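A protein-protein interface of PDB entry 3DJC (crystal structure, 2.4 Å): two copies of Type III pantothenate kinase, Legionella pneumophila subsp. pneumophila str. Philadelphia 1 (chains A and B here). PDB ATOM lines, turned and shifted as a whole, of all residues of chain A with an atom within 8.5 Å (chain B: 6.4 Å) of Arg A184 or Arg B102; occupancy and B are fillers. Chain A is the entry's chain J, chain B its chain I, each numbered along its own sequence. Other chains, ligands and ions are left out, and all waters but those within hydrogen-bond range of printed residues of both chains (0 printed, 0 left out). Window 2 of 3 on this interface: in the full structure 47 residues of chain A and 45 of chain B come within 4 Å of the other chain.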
ATOM      1  N   SER A 180     -15.835  18.051  25.027  1.00  0.00           N
ATOM      2  CA  SER A 180     -15.965  18.230  26.470  1.00  0.00           C
ATOM      3  C   SER A 180     -17.403  18.544  26.866  1.00  0.00           C
ATOM      4  O   SER A 180     -18.153  19.148  26.096  1.00  0.00           O
ATOM      5  CB  SER A 180     -15.026  19.335  26.960  1.00  0.00           C
ATOM      6  OG  SER A 180     -15.284  20.562  26.301  1.00  0.00           O
ATOM      7  N   VAL A 181     -17.776  18.122  28.071  1.00  0.00           N
ATOM      8  CA  VAL A 181     -19.119  18.347  28.607  1.00  0.00           C
ATOM      9  C   VAL A 181     -19.273  19.713  29.238  1.00  0.00           C
ATOM     10  O   VAL A 181     -20.370  20.269  29.266  1.00  0.00           O
ATOM     11  CB  VAL A 181     -19.491  17.311  29.673  1.00  0.00           C
ATOM     12  CG1 VAL A 181     -20.270  16.187  29.053  1.00  0.00           C
ATOM     13  CG2 VAL A 181     -18.243  16.810  30.394  1.00  0.00           C
ATOM     14  N   VAL A 182     -18.171  20.234  29.765  1.00  0.00           N
ATOM     15  CA  VAL A 182     -18.155  21.548  30.395  1.00  0.00           C
ATOM     16  C   VAL A 182     -18.292  22.623  29.317  1.00  0.00           C
ATOM     17  O   VAL A 182     -17.361  22.885  28.549  1.00  0.00           O
ATOM     18  CB  VAL A 182     -16.886  21.751  31.271  1.00  0.00           C
ATOM     19  CG1 VAL A 182     -16.876  23.130  31.919  1.00  0.00           C
ATOM     20  CG2 VAL A 182     -16.808  20.670  32.338  1.00  0.00           C
ATOM     21  N   GLY A 183     -19.485  23.202  29.245  1.00  0.00           N
ATOM     22  CA  GLY A 183     -19.756  24.297  28.330  1.00  0.00           C
ATOM     23  C   GLY A 183     -19.541  25.610  29.043  1.00  0.00           C
ATOM     24  O   GLY A 183     -20.124  25.853  30.097  1.00  0.00           O
ATOM     25  N   ARG A 184     -18.685  26.450  28.469  1.00  0.00           N
ATOM     26  CA  ARG A 184     -18.423  27.787  29.001  1.00  0.00           C
ATOM     27  C   ARG A 184     -19.074  28.848  28.106  1.00  0.00           C
ATOM     28  O   ARG A 184     -18.615  29.988  28.013  1.00  0.00           O
ATOM     29  CB  ARG A 184     -16.919  28.008  29.157  1.00  0.00           C
ATOM     30  CG  ARG A 184     -16.278  27.074  30.171  1.00  0.00           C
ATOM     31  CD  ARG A 184     -14.776  26.995  30.002  1.00  0.00           C
ATOM     32  NE  ARG A 184     -14.222  25.845  30.712  1.00  0.00           N
ATOM     33  CZ  ARG A 184     -13.984  24.656  30.160  1.00  0.00           C
ATOM     34  NH1 ARG A 184     -14.244  24.444  28.874  1.00  0.00           N
ATOM     35  NH2 ARG A 184     -13.478  23.676  30.897  1.00  0.00           N
ATOM     36  N   SER A 185     -20.155  28.431  27.450  1.00  0.00           N
ATOM     37  CA  SER A 185     -21.010  29.282  26.636  1.00  0.00           C
ATOM     38  C   SER A 185     -22.380  28.614  26.601  1.00  0.00           C
ATOM     39  O   SER A 185     -22.499  27.442  26.959  1.00  0.00           O
ATOM     40  CB  SER A 185     -20.452  29.409  25.217  1.00  0.00           C
ATOM     41  OG  SER A 185     -21.363  30.084  24.364  1.00  0.00           O
ATOM     42  N   THR A 186     -23.404  29.357  26.176  1.00  0.00           N
ATOM     43  CA  THR A 186     -24.753  28.814  25.978  1.00  0.00           C
ATOM     44  C   THR A 186     -24.765  27.880  24.762  1.00  0.00           C
ATOM     45  O   THR A 186     -25.452  26.854  24.757  1.00  0.00           O
ATOM     46  CB  THR A 186     -25.798  29.947  25.803  1.00  0.00           C
ATOM     47  OG1 THR A 186     -25.697  30.864  26.898  1.00  0.00           O
ATOM     48  CG2 THR A 186     -27.223  29.400  25.749  1.00  0.00           C
ATOM     49  N   ILE A 187     -23.984  28.252  23.748  1.00  0.00           N
ATOM     50  CA  ILE A 187     -23.809  27.479  22.521  1.00  0.00           C
ATOM     51  C   ILE A 187     -23.114  26.148  22.822  1.00  0.00           C
ATOM     52  O   ILE A 187     -23.524  25.094  22.335  1.00  0.00           O
ATOM     53  CB  ILE A 187     -23.010  28.304  21.464  1.00  0.00           C
ATOM     54  CG1 ILE A 187     -23.797  29.562  21.066  1.00  0.00           C
ATOM     55  CG2 ILE A 187     -22.654  27.461  20.227  1.00  0.00           C
ATOM     56  CD1 ILE A 187     -22.956  30.653  20.421  1.00  0.00           C
ATOM     57  N   GLU A 188     -22.077  26.203  23.650  1.00  0.00           N
ATOM     58  CA  GLU A 188     -21.340  25.003  24.037  1.00  0.00           C
ATOM     59  C   GLU A 188     -22.151  24.108  24.979  1.00  0.00           C
ATOM     60  O   GLU A 188     -21.946  22.898  25.003  1.00  0.00           O
ATOM     61  CB  GLU A 188     -19.995  25.375  24.666  1.00  0.00           C
ATOM     62  CG  GLU A 188     -19.009  26.008  23.692  1.00  0.00           C
ATOM     63  CD  GLU A 188     -17.955  26.863  24.377  1.00  0.00           C
ATOM     64  OE1 GLU A 188     -17.568  27.891  23.787  1.00  0.00           O
ATOM     65  OE2 GLU A 188     -17.514  26.518  25.496  1.00  0.00           O
ATOM     66  N   SER A 189     -23.068  24.705  25.739  1.00  0.00           N
ATOM     67  CA  SER A 189     -23.930  23.957  26.659  1.00  0.00           C
ATOM     68  C   SER A 189     -25.018  23.153  25.952  1.00  0.00           C
ATOM     69  O   SER A 189     -25.330  22.040  26.373  1.00  0.00           O
ATOM     70  CB  SER A 189     -24.556  24.879  27.709  1.00  0.00           C
ATOM     71  OG  SER A 189     -23.665  25.081  28.793  1.00  0.00           O
ATOM     72  N   ILE A 190     -25.592  23.714  24.889  1.00  0.00           N
ATOM     73  CA  ILE A 190     -26.577  22.993  24.068  1.00  0.00           C
ATOM     74  C   ILE A 190     -25.888  21.930  23.194  1.00  0.00           C
ATOM     75  O   ILE A 190     -26.450  20.866  22.946  1.00  0.00           O
ATOM     76  CB  ILE A 190     -27.530  23.964  23.271  1.00  0.00           C
ATOM     77  CG1 ILE A 190     -28.526  23.201  22.392  1.00  0.00           C
ATOM     78  CG2 ILE A 190     -26.750  24.962  22.436  1.00  0.00           C
ATOM     79  CD1 ILE A 190     -29.610  24.077  21.773  1.00  0.00           C
ATOM     80  N   SER A 192     -23.095  20.287  24.202  1.00  0.00           N
ATOM     81  CA  SER A 192     -22.541  19.267  25.101  1.00  0.00           C
ATOM     82  C   SER A 192     -23.617  18.446  25.801  1.00  0.00           C
ATOM     83  O   SER A 192     -23.328  17.408  26.394  1.00  0.00           O
ATOM     84  CB  SER A 192     -21.624  19.904  26.148  1.00  0.00           C
ATOM     85  OG  SER A 192     -20.514  20.535  25.538  1.00  0.00           O
ATOM     86  N   ILE B  99     -17.613  32.929  38.338  1.00  0.00           N
ATOM     87  CA  ILE B  99     -18.174  32.411  37.086  1.00  0.00           C
ATOM     88  C   ILE B  99     -17.077  32.151  36.046  1.00  0.00           C
ATOM     89  O   ILE B  99     -16.349  33.072  35.664  1.00  0.00           O
ATOM     90  CB  ILE B  99     -19.257  33.365  36.511  1.00  0.00           C
ATOM     91  CG1 ILE B  99     -20.376  33.587  37.530  1.00  0.00           C
ATOM     92  CG2 ILE B  99     -19.836  32.812  35.218  1.00  0.00           C
ATOM     93  CD1 ILE B  99     -21.304  34.743  37.192  1.00  0.00           C
ATOM     94  N   LYS B 100     -16.968  30.897  35.603  1.00  0.00           N
ATOM     95  CA  LYS B 100     -15.930  30.493  34.645  1.00  0.00           C
ATOM     96  C   LYS B 100     -16.407  30.451  33.188  1.00  0.00           C
ATOM     97  O   LYS B 100     -15.744  29.858  32.331  1.00  0.00           O
ATOM     98  CB  LYS B 100     -15.274  29.164  35.056  1.00  0.00           C
ATOM     99  CG  LYS B 100     -13.980  29.324  35.857  1.00  0.00           C
ATOM    100  CD  LYS B 100     -14.242  29.586  37.331  1.00  0.00           C
ATOM    101  CE  LYS B 100     -13.191  30.509  37.940  1.00  0.00           C
ATOM    102  NZ  LYS B 100     -13.390  31.947  37.566  1.00  0.00           N
ATOM    103  N   TYR B 101     -17.553  31.078  32.924  1.00  0.00           N
ATOM    104  CA  TYR B 101     -18.054  31.291  31.563  1.00  0.00           C
ATOM    105  C   TYR B 101     -17.172  32.281  30.798  1.00  0.00           C
ATOM    106  O   TYR B 101     -16.598  33.199  31.395  1.00  0.00           O
ATOM    107  CB  TYR B 101     -19.487  31.829  31.613  1.00  0.00           C
ATOM    108  CG  TYR B 101     -20.578  30.867  31.175  1.00  0.00           C
ATOM    109  CD1 TYR B 101     -20.661  29.577  31.696  1.00  0.00           C
ATOM    110  CD2 TYR B 101     -21.550  31.269  30.255  1.00  0.00           C
ATOM    111  CE1 TYR B 101     -21.671  28.705  31.293  1.00  0.00           C
ATOM    112  CE2 TYR B 101     -22.564  30.414  29.857  1.00  0.00           C
ATOM    113  CZ  TYR B 101     -22.619  29.134  30.373  1.00  0.00           C
ATOM    114  OH  TYR B 101     -23.626  28.288  29.969  1.00  0.00           O
ATOM    115  N   ARG B 102     -17.071  32.085  29.482  1.00  0.00           N
ATOM    116  CA  ARG B 102     -16.374  33.018  28.585  1.00  0.00           C
ATOM    117  C   ARG B 102     -17.077  34.370  28.569  1.00  0.00           C
ATOM    118  O   ARG B 102     -16.436  35.422  28.469  1.00  0.00           O
ATOM    119  CB  ARG B 102     -16.294  32.457  27.161  1.00  0.00           C
ATOM    120  CG  ARG B 102     -14.951  31.840  26.788  1.00  0.00           C
ATOM    121  CD  ARG B 102     -14.773  30.453  27.383  1.00  0.00           C
ATOM    122  NE  ARG B 102     -13.753  29.678  26.679  1.00  0.00           N
ATOM    123  CZ  ARG B 102     -13.976  28.940  25.592  1.00  0.00           C
ATOM    124  NH1 ARG B 102     -12.976  28.275  25.032  1.00  0.00           N
ATOM    125  NH2 ARG B 102     -15.189  28.865  25.059  1.00  0.00           N
ATOM    126  N   ASN B 103     -18.401  34.312  28.657  1.00  0.00           N
ATOM    127  CA  ASN B 103     -19.231  35.476  28.891  1.00  0.00           C
ATOM    128  C   ASN B 103     -20.062  35.220  30.151  1.00  0.00           C
ATOM    129  O   ASN B 103     -21.063  34.505  30.094  1.00  0.00           O
ATOM    130  CB  ASN B 103     -20.121  35.736  27.671  1.00  0.00           C
ATOM    131  CG  ASN B 103     -20.859  37.057  27.749  1.00  0.00           C
ATOM    132  OD1 ASN B 103     -20.475  37.960  28.494  1.00  0.00           O
ATOM    133  ND2 ASN B 103     -21.924  37.178  26.968  1.00  0.00           N
ATOM    134  N   PRO B 104     -19.634  35.786  31.303  1.00  0.00           N
ATOM    135  CA  PRO B 104     -20.317  35.620  32.597  1.00  0.00           C
ATOM    136  C   PRO B 104     -21.750  36.173  32.635  1.00  0.00           C
ATOM    137  O   PRO B 104     -22.533  35.788  33.506  1.00  0.00           O
ATOM    138  CB  PRO B 104     -19.425  36.405  33.569  1.00  0.00           C
ATOM    139  CG  PRO B 104     -18.105  36.501  32.891  1.00  0.00           C
ATOM    140  CD  PRO B 104     -18.430  36.624  31.439  1.00  0.00           C
ATOM    141  N   GLU B 106     -23.853  35.719  30.136  1.00  0.00           N
ATOM    142  CA  GLU B 106     -24.653  34.754  29.370  1.00  0.00           C
ATOM    143  C   GLU B 106     -25.289  33.652  30.228  1.00  0.00           C
ATOM    144  O   GLU B 106     -26.194  32.949  29.768  1.00  0.00           O
ATOM    145  CB  GLU B 106     -23.797  34.134  28.265  1.00  0.00           C
ATOM    146  CG  GLU B 106     -24.514  33.937  26.941  1.00  0.00           C
ATOM    147  CD  GLU B 106     -23.584  33.432  25.856  1.00  0.00           C
ATOM    148  OE1 GLU B 106     -23.353  34.184  24.883  1.00  0.00           O
ATOM    149  OE2 GLU B 106     -23.070  32.296  25.980  1.00  0.00           O
ATOM    150  N   LEU B 148     -18.332  26.527  36.966  1.00  0.00           N
ATOM    151  CA  LEU B 148     -17.503  26.121  35.826  1.00  0.00           C
ATOM    152  C   LEU B 148     -18.304  26.025  34.523  1.00  0.00           C
ATOM    153  O   LEU B 148     -17.728  26.053  33.429  1.00  0.00           O
ATOM    154  CB  LEU B 148     -16.787  24.797  36.124  1.00  0.00           C
ATOM    155  CG  LEU B 148     -16.053  24.679  37.469  1.00  0.00           C
ATOM    156  CD1 LEU B 148     -15.864  23.226  37.859  1.00  0.00           C
ATOM    157  CD2 LEU B 148     -14.718  25.410  37.459  1.00  0.00           C
ATOM    158  N   GLY B 149     -19.628  25.936  34.652  1.00  0.00           N
ATOM    159  CA  GLY B 149     -20.524  25.778  33.508  1.00  0.00           C
ATOM    160  C   GLY B 149     -21.147  24.395  33.493  1.00  0.00           C
ATOM    161  O   GLY B 149     -21.192  23.720  34.526  1.00  0.00           O
ATOM    162  N   GLY B 150     -21.626  23.970  32.327  1.00  0.00           N
ATOM    163  CA  GLY B 150     -22.221  22.643  32.187  1.00  0.00           C
ATOM    164  C   GLY B 150     -22.876  22.349  30.851  1.00  0.00           C
ATOM    165  O   GLY B 150     -22.270  22.543  29.796  1.00  0.00           O
ATOM    166  N   GLU B 212     -14.120  15.095  34.368  1.00  0.00           N
ATOM    167  CA  GLU B 212     -13.474  16.155  33.586  1.00  0.00           C
ATOM    168  C   GLU B 212     -13.428  17.515  34.294  1.00  0.00           C
ATOM    169  O   GLU B 212     -12.476  18.281  34.107  1.00  0.00           O
ATOM    170  CB  GLU B 212     -14.125  16.301  32.207  1.00  0.00           C
ATOM    171  CG  GLU B 212     -13.193  16.874  31.137  1.00  0.00           C
ATOM    172  CD  GLU B 212     -13.898  17.804  30.172  1.00  0.00           C
ATOM    173  OE1 GLU B 212     -13.324  18.867  29.854  1.00  0.00           O
ATOM    174  OE2 GLU B 212     -15.023  17.482  29.734  1.00  0.00           O
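The backbone carbonyl oxygen (O) of Gly B150 sits at hydrogen-bond distance from the backbone NH (N) of Gly A183 (2.9 Å). The side-chain hydroxyl (OG) of Ser A189 lies within hydrogen-bond range of the side-chain hydroxyl (OH) of Tyr B101. The backbone NH of Val A181 is in hydrogen-bond range of the side-chain carboxylate of Glu B212, 3.3 Å away. The backbone NH of Arg B102 sits at hydrogen-bond distance from the backbone carbonyl oxygen of Arg A184. OG of Ser A185 sits at hydrogen-bond distance from OE2 of Glu B106. The side-chain carboxylate of Glu B106 sits at hydrogen-bond distance from the backbone NH of Thr A186 (3.0 Å). The backbone carbonyl oxygen of Gly B150 is in hydrogen-bond range of the side-chain hydroxyl of Ser A189. NH2 of Arg B102 lies within salt-bridge range of OE1 of Glu A188 (2.9 Å). O of Gly B150 lies close to O of Val A181, 3.0 Å away. The backbone carbonyl oxygen (O) of Ser A185 is in hydrogen-bond range of the side-chain hydroxyl (OH) of Tyr B101 (3.3 Å).
OG of Ser A189 is in hydrogen-bond range of O of Ser A185 (3.2 Å). The backbone NH (N) of Arg A184 sits at hydrogen-bond distance from the side-chain carboxylate (OE2) of Glu A188 (3.2 Å). N of Ile A187 sits at hydrogen-bond distance from OG of Ser A185, 3.3 Å away. OG of Ser A192 sits at hydrogen-bond distance from O of Ser A180 (2.8 Å). O of Glu A188 sits at hydrogen-bond distance from OG of Ser A192.
Ser A180 touches Glu B212. CG1 of Val A182 touches O of Leu B148 (3.4 Å). Tyr B101 touches Gly A183. Gly A183 touches Gly B149. Lys B100 touches Arg A184 (O to CG, 3.6 Å). Arg A184 touches Tyr B101. Arg A184 touches Leu B148 (CG to O, 3.7 Å). CE2 of Tyr B101 touches N of Thr A186, at 3.9 Å.
Of chain B, only Lys B100, Tyr B101, Arg B102 and Leu B148 come within 4 Å of Arg A184. Of chain A, only Arg A184 and Glu A188 come within 4 Å of Arg B102. Of the printed residues of chain B, Ser A180 touches Glu B212. Printed residues of chain A within 4 Å of Glu B106: Ser A185 and Thr A186. Of the printed residues of chain B, Ser A185 touches Tyr B101 (3.3 Å) and Glu B106 (3.2 Å). Of the printed residues of chain A, Lys B100 touches Arg A184 (3.6 Å). Printed residues of chain B within 4 Å of Val A182: Leu B148 (3.4 Å). Asn B103 touches none of the printed residues of chain A. The nearest residue of chain B that does not touch Arg A184 is Asn B103 (4.4 Å). The nearest printed residue of chain A that does not touch Gly B150 is Val A182 (4.01 Å).
Of the 11 printed residues of chain B, 8 touch a printed residue of chain A. Hydrophobic or aromatic side chains of chain B that line the printed part of chain A: Tyr B101. Of the 12 printed residues of chain A, 9 touch a printed residue of chain B. Hydrophobic or aromatic side chains of chain A within 4 Å of the printed part of chain B: Val A181 and Val A182. Among the printed residues, 18 pairs touch across the chains.
No position is printed for both chains. Of the 18 pairs that touch across the chains among the printed residues, none has its exchanged pair printed and touching as well.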
